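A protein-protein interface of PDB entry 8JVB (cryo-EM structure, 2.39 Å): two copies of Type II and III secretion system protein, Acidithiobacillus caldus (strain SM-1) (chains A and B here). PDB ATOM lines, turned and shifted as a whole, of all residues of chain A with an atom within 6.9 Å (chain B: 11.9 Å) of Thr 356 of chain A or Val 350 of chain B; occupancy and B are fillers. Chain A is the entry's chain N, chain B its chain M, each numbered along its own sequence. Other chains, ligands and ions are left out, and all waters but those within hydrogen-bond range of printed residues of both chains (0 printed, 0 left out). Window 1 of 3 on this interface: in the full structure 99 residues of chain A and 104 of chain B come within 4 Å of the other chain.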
ATOM      1  N   PRO A 297      18.401 -20.607  -5.254  1.00  0.00           N
ATOM      2  CA  PRO A 297      19.251 -19.796  -6.131  1.00  0.00           C
ATOM      3  C   PRO A 297      18.514 -19.335  -7.378  1.00  0.00           C
ATOM      4  O   PRO A 297      17.764 -20.091  -8.000  1.00  0.00           O
ATOM      5  CB  PRO A 297      20.397 -20.753  -6.484  1.00  0.00           C
ATOM      6  CG  PRO A 297      19.795 -22.107  -6.369  1.00  0.00           C
ATOM      7  CD  PRO A 297      18.757 -22.036  -5.290  1.00  0.00           C
ATOM      8  N   ILE A 298      18.738 -18.073  -7.740  1.00  0.00           N
ATOM      9  CA  ILE A 298      18.109 -17.446  -8.896  1.00  0.00           C
ATOM     10  C   ILE A 298      19.186 -16.757  -9.725  1.00  0.00           C
ATOM     11  O   ILE A 298      20.089 -16.118  -9.174  1.00  0.00           O
ATOM     12  CB  ILE A 298      17.021 -16.431  -8.476  1.00  0.00           C
ATOM     13  CG1 ILE A 298      16.000 -17.082  -7.541  1.00  0.00           C
ATOM     14  CG2 ILE A 298      16.324 -15.852  -9.696  1.00  0.00           C
ATOM     15  CD1 ILE A 298      15.147 -18.136  -8.205  1.00  0.00           C
ATOM     16  N   SER A 349       6.502 -23.878 -12.033  1.00  0.00           N
ATOM     17  CA  SER A 349       7.953 -23.876 -12.118  1.00  0.00           C
ATOM     18  C   SER A 349       8.397 -24.211 -13.535  1.00  0.00           C
ATOM     19  O   SER A 349       7.816 -25.077 -14.194  1.00  0.00           O
ATOM     20  CB  SER A 349       8.551 -24.879 -11.131  1.00  0.00           C
ATOM     21  OG  SER A 349       8.146 -24.592  -9.806  1.00  0.00           O
ATOM     22  N   VAL A 350       9.434 -23.517 -14.001  1.00  0.00           N
ATOM     23  CA  VAL A 350       9.957 -23.721 -15.347  1.00  0.00           C
ATOM     24  C   VAL A 350      11.275 -24.478 -15.266  1.00  0.00           C
ATOM     25  O   VAL A 350      11.827 -24.667 -14.178  1.00  0.00           O
ATOM     26  CB  VAL A 350      10.127 -22.384 -16.090  1.00  0.00           C
ATOM     27  CG1 VAL A 350       8.774 -21.795 -16.432  1.00  0.00           C
ATOM     28  CG2 VAL A 350      10.933 -21.417 -15.253  1.00  0.00           C
ATOM     29  N   SER A 351      11.786 -24.917 -16.417  1.00  0.00           N
ATOM     30  CA  SER A 351      12.975 -25.757 -16.461  1.00  0.00           C
ATOM     31  C   SER A 351      14.214 -25.072 -17.018  1.00  0.00           C
ATOM     32  O   SER A 351      15.324 -25.519 -16.711  1.00  0.00           O
ATOM     33  CB  SER A 351      12.704 -27.023 -17.292  1.00  0.00           C
ATOM     34  OG  SER A 351      11.752 -27.856 -16.656  1.00  0.00           O
ATOM     35  N   LEU A 352      14.063 -24.007 -17.809  1.00  0.00           N
ATOM     36  CA  LEU A 352      15.178 -23.357 -18.493  1.00  0.00           C
ATOM     37  C   LEU A 352      15.996 -24.395 -19.258  1.00  0.00           C
ATOM     38  O   LEU A 352      15.471 -25.047 -20.165  1.00  0.00           O
ATOM     39  CB  LEU A 352      16.044 -22.583 -17.495  1.00  0.00           C
ATOM     40  CG  LEU A 352      16.917 -21.445 -18.034  1.00  0.00           C
ATOM     41  CD1 LEU A 352      16.268 -20.784 -19.239  1.00  0.00           C
ATOM     42  CD2 LEU A 352      17.198 -20.417 -16.949  1.00  0.00           C
ATOM     43  N   ASN A 353      17.275 -24.563 -18.911  1.00  0.00           N
ATOM     44  CA  ASN A 353      18.079 -25.653 -19.458  1.00  0.00           C
ATOM     45  C   ASN A 353      18.198 -26.809 -18.472  1.00  0.00           C
ATOM     46  O   ASN A 353      17.797 -27.937 -18.769  1.00  0.00           O
ATOM     47  CB  ASN A 353      19.476 -25.148 -19.843  1.00  0.00           C
ATOM     48  CG  ASN A 353      19.468 -23.718 -20.332  1.00  0.00           C
ATOM     49  OD1 ASN A 353      19.351 -22.782 -19.543  1.00  0.00           O
ATOM     50  ND2 ASN A 353      19.594 -23.539 -21.641  1.00  0.00           N
ATOM     51  N   GLY A 354      18.748 -26.537 -17.294  1.00  0.00           N
ATOM     52  CA  GLY A 354      18.749 -27.475 -16.191  1.00  0.00           C
ATOM     53  C   GLY A 354      18.630 -26.709 -14.893  1.00  0.00           C
ATOM     54  O   GLY A 354      18.578 -27.290 -13.805  1.00  0.00           O
ATOM     55  N   PHE A 355      18.587 -25.385 -15.015  1.00  0.00           N
ATOM     56  CA  PHE A 355      18.437 -24.484 -13.876  1.00  0.00           C
ATOM     57  C   PHE A 355      16.947 -24.303 -13.631  1.00  0.00           C
ATOM     58  O   PHE A 355      16.321 -23.374 -14.141  1.00  0.00           O
ATOM     59  CB  PHE A 355      19.128 -23.154 -14.146  1.00  0.00           C
ATOM     60  CG  PHE A 355      19.680 -22.496 -12.916  1.00  0.00           C
ATOM     61  CD1 PHE A 355      18.874 -21.704 -12.117  1.00  0.00           C
ATOM     62  CD2 PHE A 355      21.007 -22.662 -12.562  1.00  0.00           C
ATOM     63  CE1 PHE A 355      19.381 -21.096 -10.987  1.00  0.00           C
ATOM     64  CE2 PHE A 355      21.519 -22.053 -11.436  1.00  0.00           C
ATOM     65  CZ  PHE A 355      20.703 -21.271 -10.645  1.00  0.00           C
ATOM     66  N   THR A 356      16.370 -25.213 -12.851  1.00  0.00           N
ATOM     67  CA  THR A 356      14.955 -25.120 -12.520  1.00  0.00           C
ATOM     68  C   THR A 356      14.682 -23.834 -11.752  1.00  0.00           C
ATOM     69  O   THR A 356      15.363 -23.527 -10.770  1.00  0.00           O
ATOM     70  CB  THR A 356      14.523 -26.329 -11.693  1.00  0.00           C
ATOM     71  OG1 THR A 356      14.603 -27.512 -12.496  1.00  0.00           O
ATOM     72  CG2 THR A 356      13.099 -26.157 -11.199  1.00  0.00           C
ATOM     73  N   VAL A 357      13.692 -23.080 -12.206  1.00  0.00           N
ATOM     74  CA  VAL A 357      13.261 -21.847 -11.557  1.00  0.00           C
ATOM     75  C   VAL A 357      11.871 -22.093 -10.983  1.00  0.00           C
ATOM     76  O   VAL A 357      10.941 -22.399 -11.741  1.00  0.00           O
ATOM     77  CB  VAL A 357      13.256 -20.661 -12.533  1.00  0.00           C
ATOM     78  CG1 VAL A 357      13.225 -19.352 -11.768  1.00  0.00           C
ATOM     79  CG2 VAL A 357      14.466 -20.723 -13.443  1.00  0.00           C
ATOM     80  N   PRO A 358      11.682 -21.984  -9.673  1.00  0.00           N
ATOM     81  CA  PRO A 358      10.402 -22.345  -9.069  1.00  0.00           C
ATOM     82  C   PRO A 358       9.396 -21.201  -9.068  1.00  0.00           C
ATOM     83  O   PRO A 358       9.740 -20.021  -9.162  1.00  0.00           O
ATOM     84  CB  PRO A 358      10.802 -22.712  -7.635  1.00  0.00           C
ATOM     85  CG  PRO A 358      11.955 -21.812  -7.352  1.00  0.00           C
ATOM     86  CD  PRO A 358      12.672 -21.577  -8.662  1.00  0.00           C
ATOM     87  N   VAL B 296      30.735 -22.234   0.670  1.00  0.00           N
ATOM     88  CA  VAL B 296      30.539 -22.901  -0.614  1.00  0.00           C
ATOM     89  C   VAL B 296      30.806 -21.902  -1.733  1.00  0.00           C
ATOM     90  O   VAL B 296      30.505 -20.710  -1.583  1.00  0.00           O
ATOM     91  CB  VAL B 296      29.128 -23.499  -0.731  1.00  0.00           C
ATOM     92  CG1 VAL B 296      29.042 -24.806   0.030  1.00  0.00           C
ATOM     93  CG2 VAL B 296      28.087 -22.516  -0.229  1.00  0.00           C
ATOM     94  N   PRO B 297      31.368 -22.334  -2.860  1.00  0.00           N
ATOM     95  CA  PRO B 297      31.646 -21.398  -3.954  1.00  0.00           C
ATOM     96  C   PRO B 297      30.404 -21.099  -4.782  1.00  0.00           C
ATOM     97  O   PRO B 297      29.614 -21.990  -5.101  1.00  0.00           O
ATOM     98  CB  PRO B 297      32.703 -22.135  -4.782  1.00  0.00           C
ATOM     99  CG  PRO B 297      32.443 -23.574  -4.517  1.00  0.00           C
ATOM    100  CD  PRO B 297      31.924 -23.674  -3.115  1.00  0.00           C
ATOM    101  N   ILE B 298      30.244 -19.825  -5.131  1.00  0.00           N
ATOM    102  CA  ILE B 298      29.109 -19.343  -5.909  1.00  0.00           C
ATOM    103  C   ILE B 298      29.630 -18.483  -7.053  1.00  0.00           C
ATOM    104  O   ILE B 298      30.552 -17.681  -6.868  1.00  0.00           O
ATOM    105  CB  ILE B 298      28.118 -18.536  -5.038  1.00  0.00           C
ATOM    106  CG1 ILE B 298      27.682 -19.346  -3.815  1.00  0.00           C
ATOM    107  CG2 ILE B 298      26.905 -18.114  -5.851  1.00  0.00           C
ATOM    108  CD1 ILE B 298      26.834 -20.549  -4.149  1.00  0.00           C
ATOM    109  N   LEU B 299      29.040 -18.651  -8.234  1.00  0.00           N
ATOM    110  CA  LEU B 299      29.388 -17.831  -9.389  1.00  0.00           C
ATOM    111  C   LEU B 299      28.569 -16.546  -9.367  1.00  0.00           C
ATOM    112  O   LEU B 299      27.340 -16.586  -9.464  1.00  0.00           O
ATOM    113  CB  LEU B 299      29.143 -18.597 -10.687  1.00  0.00           C
ATOM    114  CG  LEU B 299      29.800 -19.970 -10.815  1.00  0.00           C
ATOM    115  CD1 LEU B 299      29.137 -20.778 -11.916  1.00  0.00           C
ATOM    116  CD2 LEU B 299      31.289 -19.824 -11.073  1.00  0.00           C
ATOM    117  N   ILE B 344      22.614 -26.924   4.313  1.00  0.00           N
ATOM    118  CA  ILE B 344      22.493 -27.183   2.883  1.00  0.00           C
ATOM    119  C   ILE B 344      21.330 -28.136   2.649  1.00  0.00           C
ATOM    120  O   ILE B 344      21.227 -29.181   3.299  1.00  0.00           O
ATOM    121  CB  ILE B 344      23.804 -27.753   2.320  1.00  0.00           C
ATOM    122  CG1 ILE B 344      24.859 -26.651   2.222  1.00  0.00           C
ATOM    123  CG2 ILE B 344      23.573 -28.388   0.961  1.00  0.00           C
ATOM    124  CD1 ILE B 344      26.234 -27.158   1.885  1.00  0.00           C
ATOM    125  N   ASP B 345      20.448 -27.774   1.720  1.00  0.00           N
ATOM    126  CA  ASP B 345      19.265 -28.571   1.423  1.00  0.00           C
ATOM    127  C   ASP B 345      19.395 -29.212   0.049  1.00  0.00           C
ATOM    128  O   ASP B 345      19.426 -28.492  -0.963  1.00  0.00           O
ATOM    129  CB  ASP B 345      18.008 -27.703   1.488  1.00  0.00           C
ATOM    130  CG  ASP B 345      16.762 -28.451   1.073  1.00  0.00           C
ATOM    131  OD1 ASP B 345      16.552 -29.578   1.563  1.00  0.00           O
ATOM    132  OD2 ASP B 345      15.992 -27.909   0.257  1.00  0.00           O
ATOM    133  N   PRO B 346      19.477 -30.541  -0.047  1.00  0.00           N
ATOM    134  CA  PRO B 346      19.598 -31.174  -1.369  1.00  0.00           C
ATOM    135  C   PRO B 346      18.345 -31.068  -2.221  1.00  0.00           C
ATOM    136  O   PRO B 346      18.437 -31.226  -3.444  1.00  0.00           O
ATOM    137  CB  PRO B 346      19.916 -32.635  -1.030  1.00  0.00           C
ATOM    138  CG  PRO B 346      19.330 -32.839   0.323  1.00  0.00           C
ATOM    139  CD  PRO B 346      19.449 -31.528   1.045  1.00  0.00           C
ATOM    140  N   ALA B 347      17.182 -30.807  -1.621  1.00  0.00           N
ATOM    141  CA  ALA B 347      15.937 -30.810  -2.381  1.00  0.00           C
ATOM    142  C   ALA B 347      15.871 -29.645  -3.361  1.00  0.00           C
ATOM    143  O   ALA B 347      15.355 -29.794  -4.474  1.00  0.00           O
ATOM    144  CB  ALA B 347      14.743 -30.777  -1.430  1.00  0.00           C
ATOM    145  N   THR B 348      16.382 -28.478  -2.971  1.00  0.00           N
ATOM    146  CA  THR B 348      16.280 -27.276  -3.786  1.00  0.00           C
ATOM    147  C   THR B 348      17.603 -26.890  -4.437  1.00  0.00           C
ATOM    148  O   THR B 348      17.789 -25.725  -4.801  1.00  0.00           O
ATOM    149  CB  THR B 348      15.744 -26.113  -2.952  1.00  0.00           C
ATOM    150  OG1 THR B 348      16.619 -25.872  -1.845  1.00  0.00           O
ATOM    151  CG2 THR B 348      14.353 -26.432  -2.431  1.00  0.00           C
ATOM    152  N   SER B 349      18.523 -27.836  -4.587  1.00  0.00           N
ATOM    153  CA  SER B 349      19.797 -27.571  -5.237  1.00  0.00           C
ATOM    154  C   SER B 349      19.693 -27.845  -6.731  1.00  0.00           C
ATOM    155  O   SER B 349      19.058 -28.813  -7.155  1.00  0.00           O
ATOM    156  CB  SER B 349      20.901 -28.432  -4.623  1.00  0.00           C
ATOM    157  OG  SER B 349      21.012 -28.200  -3.231  1.00  0.00           O
ATOM    158  N   VAL B 350      20.322 -26.981  -7.527  1.00  0.00           N
ATOM    159  CA  VAL B 350      20.293 -27.110  -8.979  1.00  0.00           C
ATOM    160  C   VAL B 350      21.644 -27.612  -9.465  1.00  0.00           C
ATOM    161  O   VAL B 350      22.608 -27.679  -8.695  1.00  0.00           O
ATOM    162  CB  VAL B 350      19.920 -25.777  -9.652  1.00  0.00           C
ATOM    163  CG1 VAL B 350      18.462 -25.451  -9.399  1.00  0.00           C
ATOM    164  CG2 VAL B 350      20.808 -24.665  -9.146  1.00  0.00           C
ATOM    165  N   SER B 351      21.726 -27.971 -10.748  1.00  0.00           N
ATOM    166  CA  SER B 351      22.926 -28.580 -11.304  1.00  0.00           C
ATOM    167  C   SER B 351      23.702 -27.691 -12.264  1.00  0.00           C
ATOM    168  O   SER B 351      24.903 -27.922 -12.443  1.00  0.00           O
ATOM    169  CB  SER B 351      22.573 -29.888 -12.031  1.00  0.00           C
ATOM    170  OG  SER B 351      22.112 -30.870 -11.121  1.00  0.00           O
ATOM    171  N   LEU B 352      23.067 -26.685 -12.869  1.00  0.00           N
ATOM    172  CA  LEU B 352      23.687 -25.855 -13.898  1.00  0.00           C
ATOM    173  C   LEU B 352      24.300 -26.739 -14.980  1.00  0.00           C
ATOM    174  O   LEU B 352      23.581 -27.492 -15.643  1.00  0.00           O
ATOM    175  CB  LEU B 352      24.731 -24.919 -13.278  1.00  0.00           C
ATOM    176  CG  LEU B 352      25.103 -23.650 -14.052  1.00  0.00           C
ATOM    177  CD1 LEU B 352      23.925 -23.139 -14.865  1.00  0.00           C
ATOM    178  CD2 LEU B 352      25.609 -22.569 -13.110  1.00  0.00           C
ATOM    179  N   ASN B 353      25.620 -26.664 -15.175  1.00  0.00           N
ATOM    180  CA  ASN B 353      26.317 -27.599 -16.056  1.00  0.00           C
ATOM    181  C   ASN B 353      27.018 -28.697 -15.263  1.00  0.00           C
ATOM    182  O   ASN B 353      26.735 -29.884 -15.442  1.00  0.00           O
ATOM    183  CB  ASN B 353      27.336 -26.855 -16.930  1.00  0.00           C
ATOM    184  CG  ASN B 353      26.885 -25.459 -17.294  1.00  0.00           C
ATOM    185  OD1 ASN B 353      26.931 -24.546 -16.471  1.00  0.00           O
ATOM    186  ND2 ASN B 353      26.450 -25.282 -18.533  1.00  0.00           N
ATOM    187  N   GLY B 354      27.935 -28.309 -14.383  1.00  0.00           N
ATOM    188  CA  GLY B 354      28.537 -29.212 -13.425  1.00  0.00           C
ATOM    189  C   GLY B 354      28.811 -28.459 -12.142  1.00  0.00           C
ATOM    190  O   GLY B 354      29.296 -29.020 -11.157  1.00  0.00           O
ATOM    191  N   PHE B 355      28.493 -27.166 -12.163  1.00  0.00           N
ATOM    192  CA  PHE B 355      28.653 -26.289 -11.007  1.00  0.00           C
ATOM    193  C   PHE B 355      27.376 -26.378 -10.185  1.00  0.00           C
ATOM    194  O   PHE B 355      26.447 -25.587 -10.355  1.00  0.00           O
ATOM    195  CB  PHE B 355      28.937 -24.860 -11.450  1.00  0.00           C
ATOM    196  CG  PHE B 355      29.808 -24.091 -10.502  1.00  0.00           C
ATOM    197  CD1 PHE B 355      29.261 -23.445  -9.407  1.00  0.00           C
ATOM    198  CD2 PHE B 355      31.173 -24.005 -10.710  1.00  0.00           C
ATOM    199  CE1 PHE B 355      30.060 -22.736  -8.534  1.00  0.00           C
ATOM    200  CE2 PHE B 355      31.976 -23.295  -9.842  1.00  0.00           C
ATOM    201  CZ  PHE B 355      31.419 -22.661  -8.751  1.00  0.00           C
ATOM    202  N   THR B 356      27.323 -27.364  -9.294  1.00  0.00           N
ATOM    203  CA  THR B 356      26.164 -27.525  -8.429  1.00  0.00           C
ATOM    204  C   THR B 356      25.999 -26.297  -7.544  1.00  0.00           C
ATOM    205  O   THR B 356      26.950 -25.854  -6.893  1.00  0.00           O
ATOM    206  CB  THR B 356      26.314 -28.778  -7.568  1.00  0.00           C
ATOM    207  OG1 THR B 356      26.272 -29.941  -8.405  1.00  0.00           O
ATOM    208  CG2 THR B 356      25.197 -28.860  -6.546  1.00  0.00           C
ATOM    209  N   VAL B 357      24.795 -25.744  -7.529  1.00  0.00           N
ATOM    210  CA  VAL B 357      24.449 -24.599  -6.694  1.00  0.00           C
ATOM    211  C   VAL B 357      23.468 -25.085  -5.634  1.00  0.00           C
ATOM    212  O   VAL B 357      22.382 -25.568  -5.981  1.00  0.00           O
ATOM    213  CB  VAL B 357      23.851 -23.451  -7.519  1.00  0.00           C
ATOM    214  CG1 VAL B 357      23.899 -22.157  -6.731  1.00  0.00           C
ATOM    215  CG2 VAL B 357      24.591 -23.307  -8.836  1.00  0.00           C
ATOM    216  N   PRO B 358      23.797 -24.989  -4.352  1.00  0.00           N
ATOM    217  CA  PRO B 358      22.946 -25.567  -3.314  1.00  0.00           C
ATOM    218  C   PRO B 358      21.842 -24.626  -2.852  1.00  0.00           C
ATOM    219  O   PRO B 358      21.909 -23.405  -3.006  1.00  0.00           O
ATOM    220  CB  PRO B 358      23.941 -25.830  -2.177  1.00  0.00           C
ATOM    221  CG  PRO B 358      24.935 -24.730  -2.320  1.00  0.00           C
ATOM    222  CD  PRO B 358      25.021 -24.391  -3.790  1.00  0.00           C
ATOM    223  N   GLY B 359      20.803 -25.235  -2.281  1.00  0.00           N
ATOM    224  CA  GLY B 359      19.781 -24.512  -1.561  1.00  0.00           C
ATOM    225  C   GLY B 359      19.955 -24.692  -0.062  1.00  0.00           C
ATOM    226  O   GLY B 359      20.707 -25.540   0.404  1.00  0.00           O
ATOM    227  N   PHE B 360      19.233 -23.875   0.697  1.00  0.00           N
ATOM    228  CA  PHE B 360      19.437 -23.806   2.134  1.00  0.00           C
ATOM    229  C   PHE B 360      18.115 -23.847   2.886  1.00  0.00           C
ATOM    230  O   PHE B 360      17.072 -23.446   2.368  1.00  0.00           O
ATOM    231  CB  PHE B 360      20.207 -22.541   2.520  1.00  0.00           C
ATOM    232  CG  PHE B 360      21.586 -22.477   1.939  1.00  0.00           C
ATOM    233  CD1 PHE B 360      22.634 -23.157   2.531  1.00  0.00           C
ATOM    234  CD2 PHE B 360      21.834 -21.742   0.793  1.00  0.00           C
ATOM    235  CE1 PHE B 360      23.902 -23.103   1.995  1.00  0.00           C
ATOM    236  CE2 PHE B 360      23.101 -21.685   0.253  1.00  0.00           C
ATOM    237  CZ  PHE B 360      24.135 -22.366   0.855  1.00  0.00           C
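Of the 12 printed residues of chain A, 3 touch a printed residue of chain B.
Hydrophobic or aromatic side chains of chain A within 4 Å of the printed part of chain B: Pro 297 and Phe 355.
Hydrophobic or aromatic side chains of chain B within 4 Å of the printed part of chain A: Val 350, Leu 352 and Val 357.
Pro 297 of chain A touches Val 357 of chain B, but with the chains exchanged Val 357 of chain A does not touch Pro 297 of chain B (17.3 Å).
Phe 355 of chain A touches Val 350 of chain B, but with the chains exchanged Val 350 of chain A does not touch Phe 355 of chain B (15.1 Å).
Phe 355 of chain A touches Leu 352 of chain B, but with the chains exchanged Leu 352 of chain A does not touch Phe 355 of chain B (12.5 Å).
Thr 356 of chain A touches Val 350 of chain B, but with the chains exchanged Val 350 of chain A does not touch Thr 356 of chain B (15.7 Å).
Positions printed for both chains: 297, 298, 349, 350, 351, 352, 353, 354, 355, 356, 357 and 358.
Of the printed residues of chain B, Thr 356 of chain A touches Val 350.
Val 350 of chain B touches just these residues of chain A: Pro 297, Phe 355 and Thr 356.
Val 350 of chain A touches none of the printed residues of chain B.
No residue of chain B comes within 4 Å of Ser 351 of chain A.
No residue of chain B comes within 4 Å of Gly 354 of chain A.
Of chain B, only Val 350 and Leu 352 come within 4 Å of Phe 355 of chain A.
No residue of chain B comes within 4 Å of Val 357 of chain A.
Of the printed residues of chain A, Leu 352 of chain B touches Phe 355 (3.7 Å).
Of the printed residues of chain A, Val 357 of chain B touches Pro 297.
Of the printed residues of chain A, Thr 348 of chain B touches Pro 297 (3.8 Å).
Pro 358 of chain B touches none of the printed residues of chain A.
The nearest residue of chain A that does not touch Val 350 of chain B is Gly 354 of chain A (4.6 Å).
The nearest printed residue of chain A that does not touch Val 357 of chain B is Phe 355 of chain A (4.2 Å).
The backbone carbonyl oxygen (O) of Val 357 of chain B lies within hydrogen-bond range of the backbone NH (N) of Val 350 of chain B (2.9 Å).
The side-chain carboxylate (OD2) of Asp 345 of chain B lies within hydrogen-bond range of the side-chain hydroxyl (OG1) of Thr 348 of chain B, 3.0 Å away.
Among the printed residues, merely in contact across the chains: Pro 297 of chain A with Thr 348 of chain B (3.8 Å), Pro 297 of chain A with Val 350 of chain B (3.9 Å), Pro 297 of chain A with Val 357 of chain B (3.8 Å), Phe 355 of chain A with Val 350 of chain B (3.5 Å), Phe 355 of chain A with Leu 352 of chain B (3.7 Å) and Thr 356 of chain A with Val 350 of chain B (3.9 Å).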
